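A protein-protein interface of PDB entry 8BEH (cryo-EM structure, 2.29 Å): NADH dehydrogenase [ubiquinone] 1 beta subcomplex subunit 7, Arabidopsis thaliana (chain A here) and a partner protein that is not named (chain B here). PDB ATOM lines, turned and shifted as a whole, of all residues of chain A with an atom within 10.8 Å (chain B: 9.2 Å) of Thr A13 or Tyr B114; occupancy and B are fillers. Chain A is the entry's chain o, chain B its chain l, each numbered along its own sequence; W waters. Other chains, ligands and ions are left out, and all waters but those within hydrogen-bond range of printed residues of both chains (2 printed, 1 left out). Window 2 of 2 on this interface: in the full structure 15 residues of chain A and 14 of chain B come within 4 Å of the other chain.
Water W2 bridges the side-chain carboxylate of Asp A28 (2.8 Å) and the side-chain hydroxyl of Tyr B112 (3.5 Å).
Water W1 lies within hydrogen-bond range of NH1 of Arg A27 (2.9 Å), O of Gln A14 (3.1 Å) and OE2 of Glu B120 (3.4 Å).
The backbone carbonyl oxygen (O) of Ala A12 sits at hydrogen-bond distance from the side-chain hydroxyl (OH) of Tyr B114, at 3.1 Å.
The side-chain amide nitrogen (NE2) of Gln A14 lies within hydrogen-bond range of the side-chain carboxylate (OE2) of Glu B120, at 2.8 Å.
Tyr B114 touches Met A10.
OH of Tyr B114 touches CA of Thr A13 (3.6 Å).
Gln A14 touches Tyr B114.
Met A17 touches Tyr B114.
Leu A24 touches Leu B117 (O to CD1, 3.4 Å).
Glu B120 touches Leu A24 (O to CD1, 3.7 Å).
Leu A24 touches Leu B121.
Arg A27 touches Pro B113.
Arg A27 touches Glu B120 (NH1 to CG, 3.7 Å).
CB of Pro B113 touches CE of Met A29, at 3.9 Å.
Of the 25 printed residues of chain A, 8 touch a printed residue of chain B.
Hydrophobic or aromatic side chains of chain A within 4 Å of the printed part of chain B: Met A10, Met A17, Leu A24 and Met A29.
Among the printed residues, no Asp or Glu carboxylate lies within 4 Å of a Lys or Arg side-chain nitrogen of the other chain.
Of the printed residues of chain B, Thr A13 touches Tyr B114.
Tyr B114 touches just these residues of chain A: Met A10, Ala A12, Thr A13, Gln A14 and Met A17.
Gln A14 touches two residues of chain B.
No residue of chain A comes within 4 Å of Asp B115.
Of the printed residues of chain B, Met A29 touches Pro B113 (3.9 Å).
Of the printed residues of chain A, Tyr B112 touches Arg A27.
Printed residues of chain A within 4 Å of Glu B120: Gln A14, Leu A24 and Arg A27.
Printed residues of chain B within 4 Å of Met A10: Pro B113 and Tyr B114.
The nearest residue of chain A that does not touch Tyr B114 is Ile A11 (5.5 Å).
A ring nitrogen (ND1) of His A32 is in hydrogen-bond range of the backbone carbonyl oxygen (O) of Met A29, 3.1 Å away.
O of Gln A14 is in hydrogen-bond range of OG of Ser A18, at 3.4 Å.
The side-chain hydroxyl of Thr A13 lies within hydrogen-bond range of the backbone NH of Glu A16.
O of Met A17 lies within hydrogen-bond range of N of Ile A22, at 3.2 Å.
The backbone NH (N) of Tyr B112 sits at hydrogen-bond distance from the side-chain amide oxygen (OD1) of Asn B116 (3.2 Å).
OG1 of Thr A13 sits close to N of Glu A15 (3.4 Å).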
ATOM      1  N   LYS A   9       8.620 -14.183 -32.015  1.00  0.00           N
ATOM      2  CA  LYS A   9       8.543 -15.524 -31.463  1.00  0.00           C
ATOM      3  C   LYS A   9       9.877 -15.887 -30.829  1.00  0.00           C
ATOM      4  O   LYS A   9      10.931 -15.380 -31.220  1.00  0.00           O
ATOM      5  CB  LYS A   9       8.176 -16.547 -32.542  1.00  0.00           C
ATOM      6  CG  LYS A   9       6.863 -16.260 -33.250  1.00  0.00           C
ATOM      7  CD  LYS A   9       5.787 -15.799 -32.286  1.00  0.00           C
ATOM      8  CE  LYS A   9       4.488 -15.503 -33.012  1.00  0.00           C
ATOM      9  NZ  LYS A   9       4.407 -16.213 -34.316  1.00  0.00           N
ATOM     10  N   MET A  10       9.823 -16.770 -29.836  1.00  0.00           N
ATOM     11  CA  MET A  10      11.034 -17.157 -29.124  1.00  0.00           C
ATOM     12  C   MET A  10      11.966 -17.955 -30.023  1.00  0.00           C
ATOM     13  O   MET A  10      11.560 -18.936 -30.651  1.00  0.00           O
ATOM     14  CB  MET A  10      10.691 -17.959 -27.874  1.00  0.00           C
ATOM     15  CG  MET A  10      11.885 -18.154 -26.970  1.00  0.00           C
ATOM     16  SD  MET A  10      12.325 -16.667 -26.052  1.00  0.00           S
ATOM     17  CE  MET A  10      13.879 -17.188 -25.334  1.00  0.00           C
ATOM     18  N   ILE A  11      13.224 -17.537 -30.065  1.00  0.00           N
ATOM     19  CA  ILE A  11      14.241 -18.154 -30.903  1.00  0.00           C
ATOM     20  C   ILE A  11      15.231 -18.954 -30.069  1.00  0.00           C
ATOM     21  O   ILE A  11      15.531 -20.107 -30.378  1.00  0.00           O
ATOM     22  CB  ILE A  11      14.969 -17.088 -31.753  1.00  0.00           C
ATOM     23  CG1 ILE A  11      14.040 -16.547 -32.838  1.00  0.00           C
ATOM     24  CG2 ILE A  11      16.236 -17.651 -32.351  1.00  0.00           C
ATOM     25  CD1 ILE A  11      14.332 -15.113 -33.227  1.00  0.00           C
ATOM     26  N   ALA A  12      15.748 -18.354 -29.004  1.00  0.00           N
ATOM     27  CA  ALA A  12      16.692 -19.047 -28.143  1.00  0.00           C
ATOM     28  C   ALA A  12      15.978 -20.162 -27.395  1.00  0.00           C
ATOM     29  O   ALA A  12      14.878 -19.965 -26.871  1.00  0.00           O
ATOM     30  CB  ALA A  12      17.339 -18.067 -27.166  1.00  0.00           C
ATOM     31  N   THR A  13      16.587 -21.339 -27.375  1.00  0.00           N
ATOM     32  CA  THR A  13      16.045 -22.447 -26.606  1.00  0.00           C
ATOM     33  C   THR A  13      16.435 -22.313 -25.137  1.00  0.00           C
ATOM     34  O   THR A  13      17.253 -21.476 -24.753  1.00  0.00           O
ATOM     35  CB  THR A  13      16.534 -23.784 -27.158  1.00  0.00           C
ATOM     36  OG1 THR A  13      17.900 -23.989 -26.774  1.00  0.00           O
ATOM     37  CG2 THR A  13      16.419 -23.813 -28.670  1.00  0.00           C
ATOM     38  N   GLN A  14      15.819 -23.154 -24.307  1.00  0.00           N
ATOM     39  CA  GLN A  14      16.170 -23.176 -22.893  1.00  0.00           C
ATOM     40  C   GLN A  14      17.611 -23.626 -22.695  1.00  0.00           C
ATOM     41  O   GLN A  14      18.339 -23.066 -21.865  1.00  0.00           O
ATOM     42  CB  GLN A  14      15.215 -24.088 -22.131  1.00  0.00           C
ATOM     43  CG  GLN A  14      13.966 -23.402 -21.653  1.00  0.00           C
ATOM     44  CD  GLN A  14      12.761 -24.315 -21.615  1.00  0.00           C
ATOM     45  OE1 GLN A  14      12.579 -25.165 -22.482  1.00  0.00           O
ATOM     46  NE2 GLN A  14      11.941 -24.160 -20.585  1.00  0.00           N
ATOM     47  N   GLU A  15      18.038 -24.627 -23.465  1.00  0.00           N
ATOM     48  CA  GLU A  15      19.397 -25.139 -23.350  1.00  0.00           C
ATOM     49  C   GLU A  15      20.424 -24.064 -23.676  1.00  0.00           C
ATOM     50  O   GLU A  15      21.438 -23.938 -22.982  1.00  0.00           O
ATOM     51  CB  GLU A  15      19.561 -26.359 -24.261  1.00  0.00           C
ATOM     52  CG  GLU A  15      20.991 -26.867 -24.454  1.00  0.00           C
ATOM     53  CD  GLU A  15      21.789 -26.058 -25.465  1.00  0.00           C
ATOM     54  OE1 GLU A  15      21.274 -25.820 -26.577  1.00  0.00           O
ATOM     55  OE2 GLU A  15      22.925 -25.654 -25.140  1.00  0.00           O
ATOM     56  N   GLU A  16      20.187 -23.289 -24.734  1.00  0.00           N
ATOM     57  CA  GLU A  16      21.132 -22.247 -25.113  1.00  0.00           C
ATOM     58  C   GLU A  16      21.229 -21.171 -24.039  1.00  0.00           C
ATOM     59  O   GLU A  16      22.328 -20.714 -23.705  1.00  0.00           O
ATOM     60  CB  GLU A  16      20.723 -21.637 -26.453  1.00  0.00           C
ATOM     61  CG  GLU A  16      20.917 -22.559 -27.634  1.00  0.00           C
ATOM     62  CD  GLU A  16      19.972 -22.246 -28.774  1.00  0.00           C
ATOM     63  OE1 GLU A  16      19.524 -21.091 -28.877  1.00  0.00           O
ATOM     64  OE2 GLU A  16      19.671 -23.161 -29.565  1.00  0.00           O
ATOM     65  N   MET A  17      20.088 -20.760 -23.484  1.00  0.00           N
ATOM     66  CA  MET A  17      20.098 -19.724 -22.458  1.00  0.00           C
ATOM     67  C   MET A  17      20.781 -20.208 -21.185  1.00  0.00           C
ATOM     68  O   MET A  17      21.478 -19.434 -20.522  1.00  0.00           O
ATOM     69  CB  MET A  17      18.674 -19.251 -22.171  1.00  0.00           C
ATOM     70  CG  MET A  17      18.116 -18.361 -23.271  1.00  0.00           C
ATOM     71  SD  MET A  17      16.513 -17.643 -22.897  1.00  0.00           S
ATOM     72  CE  MET A  17      15.525 -19.112 -22.670  1.00  0.00           C
ATOM     73  N   SER A  18      20.593 -21.484 -20.828  1.00  0.00           N
ATOM     74  CA  SER A  18      21.285 -22.032 -19.663  1.00  0.00           C
ATOM     75  C   SER A  18      22.785 -22.156 -19.910  1.00  0.00           C
ATOM     76  O   SER A  18      23.591 -21.880 -19.015  1.00  0.00           O
ATOM     77  CB  SER A  18      20.698 -23.391 -19.287  1.00  0.00           C
ATOM     78  OG  SER A  18      19.449 -23.252 -18.642  1.00  0.00           O
ATOM     79  N   ALA A  19      23.178 -22.591 -21.112  1.00  0.00           N
ATOM     80  CA  ALA A  19      24.596 -22.718 -21.427  1.00  0.00           C
ATOM     81  C   ALA A  19      25.294 -21.369 -21.437  1.00  0.00           C
ATOM     82  O   ALA A  19      26.444 -21.268 -21.002  1.00  0.00           O
ATOM     83  CB  ALA A  19      24.781 -23.415 -22.773  1.00  0.00           C
ATOM     84  N   ALA A  20      24.627 -20.330 -21.935  1.00  0.00           N
ATOM     85  CA  ALA A  20      25.191 -18.988 -21.923  1.00  0.00           C
ATOM     86  C   ALA A  20      25.101 -18.322 -20.557  1.00  0.00           C
ATOM     87  O   ALA A  20      25.567 -17.187 -20.411  1.00  0.00           O
ATOM     88  CB  ALA A  20      24.502 -18.115 -22.973  1.00  0.00           C
ATOM     89  N   LYS A  21      24.498 -18.917 -19.564  1.00  0.00           N
ATOM     90  CA  LYS A  21      24.315 -18.379 -18.168  1.00  0.00           C
ATOM     91  C   LYS A  21      23.631 -17.011 -18.141  1.00  0.00           C
ATOM     92  O   LYS A  21      24.098 -16.186 -17.414  1.00  0.00           O
ATOM     93  CB  LYS A  21      25.654 -18.482 -17.415  1.00  0.00           C
ATOM     94  CG  LYS A  21      25.942 -19.872 -16.874  1.00  0.00           C
ATOM     95  CD  LYS A  21      27.380 -20.299 -16.944  1.00  0.00           C
ATOM     96  CE  LYS A  21      28.239 -19.743 -15.836  1.00  0.00           C
ATOM     97  NZ  LYS A  21      29.348 -20.666 -15.497  1.00  0.00           N
ATOM     98  N   ILE A  22      22.509 -16.857 -18.839  1.00  0.00           N
ATOM     99  CA  ILE A  22      21.740 -15.591 -18.818  1.00  0.00           C
ATOM    100  C   ILE A  22      21.007 -15.422 -17.490  1.00  0.00           C
ATOM    101  O   ILE A  22      20.333 -16.320 -17.113  1.00  0.00           O
ATOM    102  CB  ILE A  22      20.715 -15.508 -19.992  1.00  0.00           C
ATOM    103  CG1 ILE A  22      21.288 -16.013 -21.322  1.00  0.00           C
ATOM    104  CG2 ILE A  22      20.133 -14.123 -20.102  1.00  0.00           C
ATOM    105  CD1 ILE A  22      22.512 -15.287 -21.790  1.00  0.00           C
ATOM    106  N   LEU A  24      18.132 -14.697 -15.152  1.00  0.00           N
ATOM    107  CA  LEU A  24      16.765 -15.133 -15.443  1.00  0.00           C
ATOM    108  C   LEU A  24      15.919 -14.003 -16.041  1.00  0.00           C
ATOM    109  O   LEU A  24      15.128 -14.327 -16.878  1.00  0.00           O
ATOM    110  CB  LEU A  24      16.178 -15.685 -14.134  1.00  0.00           C
ATOM    111  CG  LEU A  24      16.846 -16.957 -13.601  1.00  0.00           C
ATOM    112  CD1 LEU A  24      16.152 -17.451 -12.346  1.00  0.00           C
ATOM    113  CD2 LEU A  24      16.924 -18.066 -14.643  1.00  0.00           C
ATOM    114  N   SER A  26      16.742 -11.683 -18.032  1.00  0.00           N
ATOM    115  CA  SER A  26      17.137 -11.387 -19.434  1.00  0.00           C
ATOM    116  C   SER A  26      16.894 -12.660 -20.277  1.00  0.00           C
ATOM    117  O   SER A  26      17.579 -12.839 -21.249  1.00  0.00           O
ATOM    118  CB  SER A  26      18.516 -10.847 -19.432  1.00  0.00           C
ATOM    119  OG  SER A  26      18.604  -9.633 -18.737  1.00  0.00           O
ATOM    120  N   ARG A  27      15.967 -13.528 -19.869  1.00  0.00           N
ATOM    121  CA  ARG A  27      15.581 -14.708 -20.704  1.00  0.00           C
ATOM    122  C   ARG A  27      14.253 -14.395 -21.430  1.00  0.00           C
ATOM    123  O   ARG A  27      13.309 -15.093 -21.243  1.00  0.00           O
ATOM    124  CB  ARG A  27      15.645 -16.016 -19.908  1.00  0.00           C
ATOM    125  CG  ARG A  27      17.005 -16.376 -19.342  1.00  0.00           C
ATOM    126  CD  ARG A  27      17.040 -17.765 -18.746  1.00  0.00           C
ATOM    127  NE  ARG A  27      18.407 -18.059 -18.381  1.00  0.00           N
ATOM    128  CZ  ARG A  27      18.863 -19.204 -17.886  1.00  0.00           C
ATOM    129  NH1 ARG A  27      18.058 -20.225 -17.683  1.00  0.00           N
ATOM    130  NH2 ARG A  27      20.141 -19.320 -17.603  1.00  0.00           N
ATOM    131  N   ASP A  28      14.248 -13.326 -22.151  1.00  0.00           N
ATOM    132  CA  ASP A  28      13.043 -12.887 -22.836  1.00  0.00           C
ATOM    133  C   ASP A  28      13.176 -13.216 -24.343  1.00  0.00           C
ATOM    134  O   ASP A  28      14.068 -13.936 -24.708  1.00  0.00           O
ATOM    135  CB  ASP A  28      12.804 -11.434 -22.436  1.00  0.00           C
ATOM    136  CG  ASP A  28      13.832 -10.407 -22.851  1.00  0.00           C
ATOM    137  OD1 ASP A  28      13.825  -9.346 -22.230  1.00  0.00           O
ATOM    138  OD2 ASP A  28      14.609 -10.663 -23.775  1.00  0.00           O
ATOM    139  N   MET A  29      12.343 -12.605 -25.164  1.00  0.00           N
ATOM    140  CA  MET A  29      12.388 -12.889 -26.595  1.00  0.00           C
ATOM    141  C   MET A  29      13.679 -12.428 -27.259  1.00  0.00           C
ATOM    142  O   MET A  29      13.973 -12.864 -28.375  1.00  0.00           O
ATOM    143  CB  MET A  29      11.206 -12.221 -27.301  1.00  0.00           C
ATOM    144  CG  MET A  29       9.852 -12.729 -26.881  1.00  0.00           C
ATOM    145  SD  MET A  29       9.238 -14.065 -27.917  1.00  0.00           S
ATOM    146  CE  MET A  29       8.727 -15.233 -26.666  1.00  0.00           C
ATOM    147  N   CYS A  30      14.460 -11.570 -26.608  1.00  0.00           N
ATOM    148  CA  CYS A  30      15.634 -10.970 -27.223  1.00  0.00           C
ATOM    149  C   CYS A  30      16.931 -11.669 -26.835  1.00  0.00           C
ATOM    150  O   CYS A  30      18.011 -11.131 -27.091  1.00  0.00           O
ATOM    151  CB  CYS A  30      15.711  -9.487 -26.858  1.00  0.00           C
ATOM    152  SG  CYS A  30      14.435  -8.454 -27.597  1.00  0.00           S
ATOM    153  N   ALA A  31      16.852 -12.859 -26.232  1.00  0.00           N
ATOM    154  CA  ALA A  31      18.041 -13.511 -25.691  1.00  0.00           C
ATOM    155  C   ALA A  31      18.947 -14.065 -26.782  1.00  0.00           C
ATOM    156  O   ALA A  31      20.169 -14.152 -26.587  1.00  0.00           O
ATOM    157  CB  ALA A  31      17.631 -14.626 -24.725  1.00  0.00           C
ATOM    158  N   HIS A  32      18.375 -14.449 -27.930  1.00  0.00           N
ATOM    159  CA  HIS A  32      19.191 -14.932 -29.037  1.00  0.00           C
ATOM    160  C   HIS A  32      20.168 -13.871 -29.522  1.00  0.00           C
ATOM    161  O   HIS A  32      21.166 -14.211 -30.161  1.00  0.00           O
ATOM    162  CB  HIS A  32      18.304 -15.400 -30.195  1.00  0.00           C
ATOM    163  CG  HIS A  32      17.484 -14.309 -30.809  1.00  0.00           C
ATOM    164  ND1 HIS A  32      16.396 -13.746 -30.177  1.00  0.00           N
ATOM    165  CD2 HIS A  32      17.599 -13.671 -31.998  1.00  0.00           C
ATOM    166  CE1 HIS A  32      15.878 -12.808 -30.948  1.00  0.00           C
ATOM    167  NE2 HIS A  32      16.586 -12.744 -32.060  1.00  0.00           N
ATOM    168  N   LEU A  33      19.899 -12.596 -29.241  1.00  0.00           N
ATOM    169  CA  LEU A  33      20.866 -11.531 -29.469  1.00  0.00           C
ATOM    170  C   LEU A  33      21.689 -11.181 -28.236  1.00  0.00           C
ATOM    171  O   LEU A  33      22.801 -10.666 -28.387  1.00  0.00           O
ATOM    172  CB  LEU A  33      20.159 -10.274 -29.984  1.00  0.00           C
ATOM    173  CG  LEU A  33      19.253 -10.546 -31.191  1.00  0.00           C
ATOM    174  CD1 LEU A  33      18.133  -9.534 -31.291  1.00  0.00           C
ATOM    175  CD2 LEU A  33      20.089 -10.563 -32.454  1.00  0.00           C
ATOM    176  N   LEU A  34      21.179 -11.448 -27.032  1.00  0.00           N
ATOM    177  CA  LEU A  34      21.980 -11.238 -25.830  1.00  0.00           C
ATOM    178  C   LEU A  34      23.191 -12.159 -25.805  1.00  0.00           C
ATOM    179  O   LEU A  34      24.276 -11.747 -25.383  1.00  0.00           O
ATOM    180  CB  LEU A  34      21.127 -11.441 -24.575  1.00  0.00           C
ATOM    181  CG  LEU A  34      21.802 -11.100 -23.235  1.00  0.00           C
ATOM    182  CD1 LEU A  34      22.500  -9.745 -23.269  1.00  0.00           C
ATOM    183  CD2 LEU A  34      20.808 -11.165 -22.086  1.00  0.00           C
ATOM    184  N   ILE A  35      23.026 -13.407 -26.255  1.00  0.00           N
ATOM    185  CA  ILE A  35      24.137 -14.364 -26.215  1.00  0.00           C
ATOM    186  C   ILE A  35      25.367 -13.857 -26.966  1.00  0.00           C
ATOM    187  O   ILE A  35      26.455 -13.806 -26.362  1.00  0.00           O
ATOM    188  CB  ILE A  35      23.661 -15.741 -26.712  1.00  0.00           C
ATOM    189  CG1 ILE A  35      22.561 -16.293 -25.801  1.00  0.00           C
ATOM    190  CG2 ILE A  35      24.818 -16.712 -26.817  1.00  0.00           C
ATOM    191  CD1 ILE A  35      21.941 -17.572 -26.296  1.00  0.00           C
ATOM    192  N   VAL B 111       5.875 -10.684 -19.983  1.00  0.00           N
ATOM    193  CA  VAL B 111       5.441 -12.098 -20.031  1.00  0.00           C
ATOM    194  C   VAL B 111       6.629 -12.811 -20.589  1.00  0.00           C
ATOM    195  O   VAL B 111       6.974 -12.589 -21.724  1.00  0.00           O
ATOM    196  CB  VAL B 111       4.121 -12.363 -20.783  1.00  0.00           C
ATOM    197  CG1 VAL B 111       3.854 -13.851 -20.904  1.00  0.00           C
ATOM    198  CG2 VAL B 111       2.949 -11.652 -20.142  1.00  0.00           C
ATOM    199  N   TYR B 112       7.202 -13.623 -19.742  1.00  0.00           N
ATOM    200  CA  TYR B 112       8.384 -14.376 -20.133  1.00  0.00           C
ATOM    201  C   TYR B 112       7.924 -15.601 -20.897  1.00  0.00           C
ATOM    202  O   TYR B 112       6.854 -16.056 -20.625  1.00  0.00           O
ATOM    203  CB  TYR B 112       9.250 -14.658 -18.893  1.00  0.00           C
ATOM    204  CG  TYR B 112      10.013 -13.438 -18.472  1.00  0.00           C
ATOM    205  CD1 TYR B 112       9.427 -12.459 -17.688  1.00  0.00           C
ATOM    206  CD2 TYR B 112      11.299 -13.237 -18.925  1.00  0.00           C
ATOM    207  CE1 TYR B 112      10.135 -11.332 -17.316  1.00  0.00           C
ATOM    208  CE2 TYR B 112      12.020 -12.122 -18.556  1.00  0.00           C
ATOM    209  CZ  TYR B 112      11.434 -11.171 -17.745  1.00  0.00           C
ATOM    210  OH  TYR B 112      12.146 -10.070 -17.400  1.00  0.00           O
ATOM    211  N   PRO B 113       8.770 -16.170 -21.761  1.00  0.00           N
ATOM    212  CA  PRO B 113       8.465 -17.435 -22.440  1.00  0.00           C
ATOM    213  C   PRO B 113       8.571 -18.644 -21.524  1.00  0.00           C
ATOM    214  O   PRO B 113       8.960 -18.528 -20.355  1.00  0.00           O
ATOM    215  CB  PRO B 113       9.514 -17.490 -23.557  1.00  0.00           C
ATOM    216  CG  PRO B 113      10.662 -16.715 -23.000  1.00  0.00           C
ATOM    217  CD  PRO B 113      10.042 -15.590 -22.227  1.00  0.00           C
ATOM    218  N   TYR B 114       8.216 -19.807 -22.064  1.00  0.00           N
ATOM    219  CA  TYR B 114       8.292 -21.092 -21.375  1.00  0.00           C
ATOM    220  C   TYR B 114       7.514 -21.063 -20.060  1.00  0.00           C
ATOM    221  O   TYR B 114       8.035 -21.354 -18.983  1.00  0.00           O
ATOM    222  CB  TYR B 114       9.749 -21.503 -21.161  1.00  0.00           C
ATOM    223  CG  TYR B 114      10.513 -21.586 -22.458  1.00  0.00           C
ATOM    224  CD1 TYR B 114      10.275 -22.616 -23.357  1.00  0.00           C
ATOM    225  CD2 TYR B 114      11.457 -20.627 -22.795  1.00  0.00           C
ATOM    226  CE1 TYR B 114      10.958 -22.694 -24.547  1.00  0.00           C
ATOM    227  CE2 TYR B 114      12.148 -20.700 -23.985  1.00  0.00           C
ATOM    228  CZ  TYR B 114      11.892 -21.738 -24.857  1.00  0.00           C
ATOM    229  OH  TYR B 114      12.578 -21.819 -26.042  1.00  0.00           O
ATOM    230  N   ASP B 115       6.232 -20.715 -20.186  1.00  0.00           N
ATOM    231  CA  ASP B 115       5.297 -20.650 -19.066  1.00  0.00           C
ATOM    232  C   ASP B 115       5.826 -19.717 -17.974  1.00  0.00           C
ATOM    233  O   ASP B 115       5.835 -20.040 -16.784  1.00  0.00           O
ATOM    234  CB  ASP B 115       5.000 -22.053 -18.527  1.00  0.00           C
ATOM    235  CG  ASP B 115       3.957 -22.055 -17.427  1.00  0.00           C
ATOM    236  OD1 ASP B 115       4.084 -22.870 -16.490  1.00  0.00           O
ATOM    237  OD2 ASP B 115       3.016 -21.237 -17.498  1.00  0.00           O
ATOM    238  N   ASN B 116       6.224 -18.534 -18.353  1.00  0.00           N
ATOM    239  CA  ASN B 116       6.779 -17.532 -17.417  1.00  0.00           C
ATOM    240  C   ASN B 116       8.022 -18.102 -16.686  1.00  0.00           C
ATOM    241  O   ASN B 116       8.189 -17.728 -15.590  1.00  0.00           O
ATOM    242  CB  ASN B 116       5.651 -16.821 -16.655  1.00  0.00           C
ATOM    243  CG  ASN B 116       5.470 -15.392 -17.092  1.00  0.00           C
ATOM    244  OD1 ASN B 116       6.331 -14.553 -16.855  1.00  0.00           O
ATOM    245  ND2 ASN B 116       4.364 -15.124 -17.759  1.00  0.00           N
ATOM    246  N   LEU B 117       8.901 -18.820 -17.421  1.00  0.00           N
ATOM    247  CA  LEU B 117      10.110 -19.396 -16.833  1.00  0.00           C
ATOM    248  C   LEU B 117       9.794 -20.187 -15.566  1.00  0.00           C
ATOM    249  O   LEU B 117      10.397 -19.990 -14.510  1.00  0.00           O
ATOM    250  CB  LEU B 117      11.155 -18.314 -16.551  1.00  0.00           C
ATOM    251  CG  LEU B 117      11.608 -17.422 -17.706  1.00  0.00           C
ATOM    252  CD1 LEU B 117      12.381 -16.231 -17.175  1.00  0.00           C
ATOM    253  CD2 LEU B 117      12.447 -18.216 -18.692  1.00  0.00           C
ATOM    254  N   ARG B 118       8.827 -21.096 -15.680  1.00  0.00           N
ATOM    255  CA  ARG B 118       8.408 -21.873 -14.522  1.00  0.00           C
ATOM    256  C   ARG B 118       9.517 -22.811 -14.064  1.00  0.00           C
ATOM    257  O   ARG B 118       9.852 -22.859 -12.876  1.00  0.00           O
ATOM    258  CB  ARG B 118       7.132 -22.653 -14.848  1.00  0.00           C
ATOM    259  CG  ARG B 118       6.647 -23.556 -13.725  1.00  0.00           C
ATOM    260  CD  ARG B 118       5.614 -24.560 -14.202  1.00  0.00           C
ATOM    261  NE  ARG B 118       6.217 -25.762 -14.762  1.00  0.00           N
ATOM    262  CZ  ARG B 118       6.297 -26.026 -16.058  1.00  0.00           C
ATOM    263  NH1 ARG B 118       5.822 -25.187 -16.964  1.00  0.00           N
ATOM    264  NH2 ARG B 118       6.872 -27.155 -16.455  1.00  0.00           N
ATOM    265  N   VAL B 119      10.113 -23.552 -14.999  1.00  0.00           N
ATOM    266  CA  VAL B 119      11.151 -24.511 -14.641  1.00  0.00           C
ATOM    267  C   VAL B 119      12.432 -23.797 -14.224  1.00  0.00           C
ATOM    268  O   VAL B 119      13.088 -24.191 -13.255  1.00  0.00           O
ATOM    269  CB  VAL B 119      11.391 -25.494 -15.802  1.00  0.00           C
ATOM    270  CG1 VAL B 119      12.498 -26.468 -15.452  1.00  0.00           C
ATOM    271  CG2 VAL B 119      10.105 -26.235 -16.136  1.00  0.00           C
ATOM    272  N   GLU B 120      12.809 -22.736 -14.943  1.00  0.00           N
ATOM    273  CA  GLU B 120      14.023 -21.997 -14.614  1.00  0.00           C
ATOM    274  C   GLU B 120      13.941 -21.312 -13.258  1.00  0.00           C
ATOM    275  O   GLU B 120      14.981 -20.989 -12.679  1.00  0.00           O
ATOM    276  CB  GLU B 120      14.328 -20.956 -15.694  1.00  0.00           C
ATOM    277  CG  GLU B 120      14.671 -21.545 -17.051  1.00  0.00           C
ATOM    278  CD  GLU B 120      13.458 -22.076 -17.783  1.00  0.00           C
ATOM    279  OE1 GLU B 120      12.328 -21.693 -17.430  1.00  0.00           O
ATOM    280  OE2 GLU B 120      13.634 -22.905 -18.691  1.00  0.00           O
ATOM    281  N   LEU B 121      12.737 -21.083 -12.743  1.00  0.00           N
ATOM    282  CA  LEU B 121      12.551 -20.460 -11.444  1.00  0.00           C
ATOM    283  C   LEU B 121      12.345 -21.484 -10.335  1.00  0.00           C
ATOM    284  O   LEU B 121      11.948 -21.110  -9.228  1.00  0.00           O
ATOM    285  CB  LEU B 121      11.376 -19.486 -11.493  1.00  0.00           C
ATOM    286  CG  LEU B 121      11.717 -18.089 -12.009  1.00  0.00           C
ATOM    287  CD1 LEU B 121      10.463 -17.273 -12.216  1.00  0.00           C
ATOM    288  CD2 LEU B 121      12.682 -17.379 -11.064  1.00  0.00           C
ATOM    289  N   GLU B 124       8.074 -27.216 -10.974  1.00  0.00           N
ATOM    290  CA  GLU B 124       8.074 -28.642 -11.289  1.00  0.00           C
ATOM    291  C   GLU B 124       8.343 -28.852 -12.774  1.00  0.00           C
ATOM    292  O   GLU B 124       7.635 -28.288 -13.614  1.00  0.00           O
ATOM    293  CB  GLU B 124       6.749 -29.282 -10.904  1.00  0.00           C
ATOM    294  CG  GLU B 124       6.893 -30.639 -10.222  1.00  0.00           C
ATOM    295  CD  GLU B 124       7.067 -31.787 -11.204  1.00  0.00           C
ATOM    296  OE1 GLU B 124       7.081 -31.539 -12.428  1.00  0.00           O
ATOM    297  OE2 GLU B 124       7.188 -32.943 -10.748  1.00  0.00           O
HETATM  298  O   HOH W   1      16.569 -21.488 -19.816  1.00  0.00           O
HETATM  299  O   HOH W   2      11.669  -8.681 -20.533  1.00  0.00           O
